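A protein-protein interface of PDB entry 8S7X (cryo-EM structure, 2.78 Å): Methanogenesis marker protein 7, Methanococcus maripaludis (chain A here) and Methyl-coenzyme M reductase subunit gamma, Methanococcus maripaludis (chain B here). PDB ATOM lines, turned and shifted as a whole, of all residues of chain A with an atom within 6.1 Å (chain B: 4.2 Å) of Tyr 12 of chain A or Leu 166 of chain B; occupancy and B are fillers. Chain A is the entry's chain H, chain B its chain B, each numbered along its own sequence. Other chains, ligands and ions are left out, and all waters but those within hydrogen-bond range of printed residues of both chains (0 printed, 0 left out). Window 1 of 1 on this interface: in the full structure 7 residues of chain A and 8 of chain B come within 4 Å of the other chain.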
ATOM      1  N   GLY A  10     -15.076  31.703  24.277  1.00  0.00           N
ATOM      2  CA  GLY A  10     -16.054  30.657  24.116  1.00  0.00           C
ATOM      3  C   GLY A  10     -16.123  29.736  25.319  1.00  0.00           C
ATOM      4  O   GLY A  10     -15.238  29.728  26.170  1.00  0.00           O
ATOM      5  N   VAL A  11     -17.196  28.951  25.375  1.00  0.00           N
ATOM      6  CA  VAL A  11     -17.364  28.002  26.468  1.00  0.00           C
ATOM      7  C   VAL A  11     -16.543  26.741  26.261  1.00  0.00           C
ATOM      8  O   VAL A  11     -16.314  25.999  27.223  1.00  0.00           O
ATOM      9  CB  VAL A  11     -18.842  27.632  26.648  1.00  0.00           C
ATOM     10  CG1 VAL A  11     -19.631  28.849  27.056  1.00  0.00           C
ATOM     11  CG2 VAL A  11     -19.397  27.050  25.368  1.00  0.00           C
ATOM     12  N   TYR A  12     -16.099  26.473  25.038  1.00  0.00           N
ATOM     13  CA  TYR A  12     -15.290  25.293  24.780  1.00  0.00           C
ATOM     14  C   TYR A  12     -13.929  25.442  25.439  1.00  0.00           C
ATOM     15  O   TYR A  12     -13.239  26.446  25.240  1.00  0.00           O
ATOM     16  CB  TYR A  12     -15.134  25.083  23.277  1.00  0.00           C
ATOM     17  CG  TYR A  12     -14.373  23.837  22.905  1.00  0.00           C
ATOM     18  CD1 TYR A  12     -14.578  22.648  23.581  1.00  0.00           C
ATOM     19  CD2 TYR A  12     -13.452  23.849  21.873  1.00  0.00           C
ATOM     20  CE1 TYR A  12     -13.885  21.511  23.244  1.00  0.00           C
ATOM     21  CE2 TYR A  12     -12.755  22.716  21.528  1.00  0.00           C
ATOM     22  CZ  TYR A  12     -12.978  21.550  22.216  1.00  0.00           C
ATOM     23  OH  TYR A  12     -12.286  20.416  21.875  1.00  0.00           O
ATOM     24  N   LYS A  13     -13.543  24.440  26.230  1.00  0.00           N
ATOM     25  CA  LYS A  13     -12.290  24.430  26.977  1.00  0.00           C
ATOM     26  C   LYS A  13     -12.176  25.601  27.943  1.00  0.00           C
ATOM     27  O   LYS A  13     -11.071  25.994  28.318  1.00  0.00           O
ATOM     28  CB  LYS A  13     -11.080  24.404  26.039  1.00  0.00           C
ATOM     29  CG  LYS A  13     -11.101  23.275  25.038  1.00  0.00           C
ATOM     30  CD  LYS A  13      -9.707  22.752  24.777  1.00  0.00           C
ATOM     31  CE  LYS A  13      -9.157  23.301  23.475  1.00  0.00           C
ATOM     32  NZ  LYS A  13      -9.197  22.293  22.385  1.00  0.00           N
ATOM     33  N   ASN A  14     -13.305  26.172  28.358  1.00  0.00           N
ATOM     34  CA  ASN A  14     -13.266  27.239  29.348  1.00  0.00           C
ATOM     35  C   ASN A  14     -12.972  26.697  30.739  1.00  0.00           C
ATOM     36  O   ASN A  14     -12.424  27.417  31.581  1.00  0.00           O
ATOM     37  CB  ASN A  14     -14.587  28.001  29.340  1.00  0.00           C
ATOM     38  CG  ASN A  14     -14.515  29.294  30.105  1.00  0.00           C
ATOM     39  OD1 ASN A  14     -13.615  30.102  29.895  1.00  0.00           O
ATOM     40  ND2 ASN A  14     -15.471  29.507  30.996  1.00  0.00           N
ATOM     41  N   ASN A  15     -13.323  25.438  30.993  1.00  0.00           N
ATOM     42  CA  ASN A  15     -13.048  24.837  32.291  1.00  0.00           C
ATOM     43  C   ASN A  15     -11.550  24.711  32.537  1.00  0.00           C
ATOM     44  O   ASN A  15     -11.085  24.883  33.668  1.00  0.00           O
ATOM     45  CB  ASN A  15     -13.734  23.477  32.394  1.00  0.00           C
ATOM     46  CG  ASN A  15     -13.320  22.535  31.288  1.00  0.00           C
ATOM     47  OD1 ASN A  15     -13.637  22.755  30.121  1.00  0.00           O
ATOM     48  ND2 ASN A  15     -12.613  21.477  31.649  1.00  0.00           N
ATOM     49  N   LEU A  36     -22.845  30.365  23.316  1.00  0.00           N
ATOM     50  CA  LEU A  36     -21.592  29.650  23.154  1.00  0.00           C
ATOM     51  C   LEU A  36     -20.396  30.484  23.572  1.00  0.00           C
ATOM     52  O   LEU A  36     -19.263  30.002  23.482  1.00  0.00           O
ATOM     53  CB  LEU A  36     -21.397  29.201  21.699  1.00  0.00           C
ATOM     54  CG  LEU A  36     -22.272  28.073  21.162  1.00  0.00           C
ATOM     55  CD1 LEU A  36     -22.348  28.152  19.652  1.00  0.00           C
ATOM     56  CD2 LEU A  36     -21.735  26.726  21.593  1.00  0.00           C
ATOM     57  N   TYR A  59      -6.680  30.313  23.764  1.00  0.00           N
ATOM     58  CA  TYR A  59      -8.075  29.938  23.587  1.00  0.00           C
ATOM     59  C   TYR A  59      -8.819  30.881  22.652  1.00  0.00           C
ATOM     60  O   TYR A  59     -10.049  30.805  22.570  1.00  0.00           O
ATOM     61  CB  TYR A  59      -8.780  29.894  24.944  1.00  0.00           C
ATOM     62  CG  TYR A  59      -8.174  28.902  25.902  1.00  0.00           C
ATOM     63  CD1 TYR A  59      -8.190  27.544  25.626  1.00  0.00           C
ATOM     64  CD2 TYR A  59      -7.563  29.324  27.069  1.00  0.00           C
ATOM     65  CE1 TYR A  59      -7.631  26.639  26.496  1.00  0.00           C
ATOM     66  CE2 TYR A  59      -6.999  28.426  27.939  1.00  0.00           C
ATOM     67  CZ  TYR A  59      -7.036  27.086  27.649  1.00  0.00           C
ATOM     68  OH  TYR A  59      -6.473  26.190  28.519  1.00  0.00           O
ATOM     69  N   SER B  93     -19.047  19.488  11.641  1.00  0.00           N
ATOM     70  CA  SER B  93     -18.476  20.709  12.184  1.00  0.00           C
ATOM     71  C   SER B  93     -17.249  21.132  11.392  1.00  0.00           C
ATOM     72  O   SER B  93     -16.487  20.306  10.893  1.00  0.00           O
ATOM     73  CB  SER B  93     -18.101  20.523  13.650  1.00  0.00           C
ATOM     74  OG  SER B  93     -17.469  21.681  14.153  1.00  0.00           O
ATOM     75  N   LEU B 164     -20.413  27.251  13.819  1.00  0.00           N
ATOM     76  CA  LEU B 164     -20.319  27.761  15.174  1.00  0.00           C
ATOM     77  C   LEU B 164     -19.233  27.024  15.942  1.00  0.00           C
ATOM     78  O   LEU B 164     -18.746  25.971  15.526  1.00  0.00           O
ATOM     79  CB  LEU B 164     -21.656  27.616  15.898  1.00  0.00           C
ATOM     80  CG  LEU B 164     -22.876  28.170  15.173  1.00  0.00           C
ATOM     81  CD1 LEU B 164     -24.096  28.062  16.054  1.00  0.00           C
ATOM     82  CD2 LEU B 164     -22.641  29.608  14.764  1.00  0.00           C
ATOM     83  N   ARG B 165     -18.842  27.599  17.073  1.00  0.00           N
ATOM     84  CA  ARG B 165     -17.865  26.950  17.929  1.00  0.00           C
ATOM     85  C   ARG B 165     -18.516  25.805  18.698  1.00  0.00           C
ATOM     86  O   ARG B 165     -19.735  25.740  18.857  1.00  0.00           O
ATOM     87  CB  ARG B 165     -17.247  27.958  18.893  1.00  0.00           C
ATOM     88  CG  ARG B 165     -16.292  28.930  18.234  1.00  0.00           C
ATOM     89  CD  ARG B 165     -16.103  30.163  19.081  1.00  0.00           C
ATOM     90  NE  ARG B 165     -17.374  30.828  19.342  1.00  0.00           N
ATOM     91  CZ  ARG B 165     -17.528  31.846  20.175  1.00  0.00           C
ATOM     92  NH1 ARG B 165     -16.509  32.347  20.849  1.00  0.00           N
ATOM     93  NH2 ARG B 165     -18.736  32.374  20.334  1.00  0.00           N
ATOM     94  N   LEU B 166     -17.679  24.888  19.172  1.00  0.00           N
ATOM     95  CA  LEU B 166     -18.166  23.752  19.932  1.00  0.00           C
ATOM     96  C   LEU B 166     -18.567  24.186  21.338  1.00  0.00           C
ATOM     97  O   LEU B 166     -18.185  25.258  21.816  1.00  0.00           O
ATOM     98  CB  LEU B 166     -17.097  22.664  19.994  1.00  0.00           C
ATOM     99  CG  LEU B 166     -16.364  22.413  18.676  1.00  0.00           C
ATOM    100  CD1 LEU B 166     -15.170  21.513  18.890  1.00  0.00           C
ATOM    101  CD2 LEU B 166     -17.297  21.812  17.651  1.00  0.00           C
ATOM    102  N   ASP B 167     -19.363  23.351  22.001  1.00  0.00           N
ATOM    103  CA  ASP B 167     -19.818  23.662  23.352  1.00  0.00           C
ATOM    104  C   ASP B 167     -18.802  23.143  24.369  1.00  0.00           C
ATOM    105  O   ASP B 167     -17.683  22.757  24.023  1.00  0.00           O
ATOM    106  CB  ASP B 167     -21.231  23.125  23.581  1.00  0.00           C
ATOM    107  CG  ASP B 167     -21.329  21.611  23.481  1.00  0.00           C
ATOM    108  OD1 ASP B 167     -20.356  20.899  23.787  1.00  0.00           O
ATOM    109  OD2 ASP B 167     -22.413  21.124  23.101  1.00  0.00           O
ATOM    110  N   GLY B 170     -17.085  19.823  23.698  1.00  0.00           N
ATOM    111  CA  GLY B 170     -16.567  19.591  22.370  1.00  0.00           C
ATOM    112  C   GLY B 170     -17.588  19.116  21.366  1.00  0.00           C
ATOM    113  O   GLY B 170     -17.198  18.613  20.307  1.00  0.00           O
ATOM    114  N   MET B 171     -18.874  19.254  21.658  1.00  0.00           N
ATOM    115  CA  MET B 171     -19.939  18.797  20.779  1.00  0.00           C
ATOM    116  C   MET B 171     -20.426  19.940  19.903  1.00  0.00           C
ATOM    117  O   MET B 171     -20.465  21.097  20.323  1.00  0.00           O
ATOM    118  CB  MET B 171     -21.104  18.232  21.591  1.00  0.00           C
ATOM    119  CG  MET B 171     -20.859  16.840  22.137  1.00  0.00           C
ATOM    120  SD  MET B 171     -22.371  15.954  22.548  1.00  0.00           S
ATOM    121  CE  MET B 171     -23.530  16.722  21.428  1.00  0.00           C
ATOM    122  N   GLU B 211      -9.237  14.737  20.561  1.00  0.00           N
ATOM    123  CA  GLU B 211      -8.954  15.825  19.631  1.00  0.00           C
ATOM    124  C   GLU B 211      -7.705  15.570  18.798  1.00  0.00           C
ATOM    125  O   GLU B 211      -7.641  15.993  17.642  1.00  0.00           O
ATOM    126  CB  GLU B 211      -8.827  17.140  20.393  1.00  0.00           C
ATOM    127  CG  GLU B 211      -8.825  18.363  19.504  1.00  0.00           C
ATOM    128  CD  GLU B 211      -8.687  19.653  20.283  1.00  0.00           C
ATOM    129  OE1 GLU B 211      -8.304  19.594  21.470  1.00  0.00           O
ATOM    130  OE2 GLU B 211      -8.957  20.727  19.706  1.00  0.00           O
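The side-chain amino group (NZ) of Lys 13 of chain A is in salt-bridge range of the side-chain carboxylate (OE1) of Glu 211 of chain B, 3.0 Å away.
The backbone NH (N) of Gly 170 of chain B sits at hydrogen-bond distance from the side-chain carboxylate (OD1) of Asp 167 of chain B (3.4 Å). The backbone NH of Met 171 of chain B lies within hydrogen-bond range of the side-chain carboxylate of Asp 167 of chain B (3.1 Å). O of Leu 36 of chain A lies within hydrogen-bond range of N of Val 11 of chain A (3.0 Å).
Among the printed residues, merely in contact across the chains: Tyr 12 of chain A with Asp 167 of chain B (3.1 Å), Tyr 12 of chain A with Leu 166 of chain B (3.4 Å), Tyr 12 of chain A with Gly 170 of chain B (3.4 Å), Leu 36 of chain A with Arg 165 of chain B (3.5 Å), Gly 10 of chain A with Arg 165 of chain B (3.7 Å), Leu 36 of chain A with Leu 166 of chain B (3.8 Å), Leu 36 of chain A with Leu 164 of chain B (3.9 Å), Val 11 of chain A with Asp 167 of chain B (3.96 Å) and Tyr 12 of chain A with Glu 211 of chain B (3.99 Å).
Of the printed residues of chain B, Tyr 12 of chain A touches Leu 166, Asp 167, Gly 170 and Glu 211. Of chain A, only Tyr 12 (3.4 Å) and Leu 36 (3.8 Å) come within 4 Å of Leu 166 of chain B. Of the printed residues of chain A, Asp 167 of chain B touches Val 11 (3.96 Å) and Tyr 12 (3.1 Å). Of the printed residues of chain B, Val 11 of chain A touches Asp 167 (3.96 Å). Of the printed residues of chain A, Arg 165 of chain B touches Gly 10 (3.7 Å) and Leu 36 (3.5 Å). Of the printed residues of chain B, Leu 36 of chain A touches Leu 164, Arg 165 and Leu 166. Printed residues of chain A within 4 Å of Gly 170 of chain B: Tyr 12. The nearest printed residue of chain B that does not touch Gly 10 of chain A is Leu 166 of chain B (6.0 Å).
Of the 8 printed residues of chain A, 5 touch a printed residue of chain B. Of the 8 printed residues of chain B, 6 touch a printed residue of chain A.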
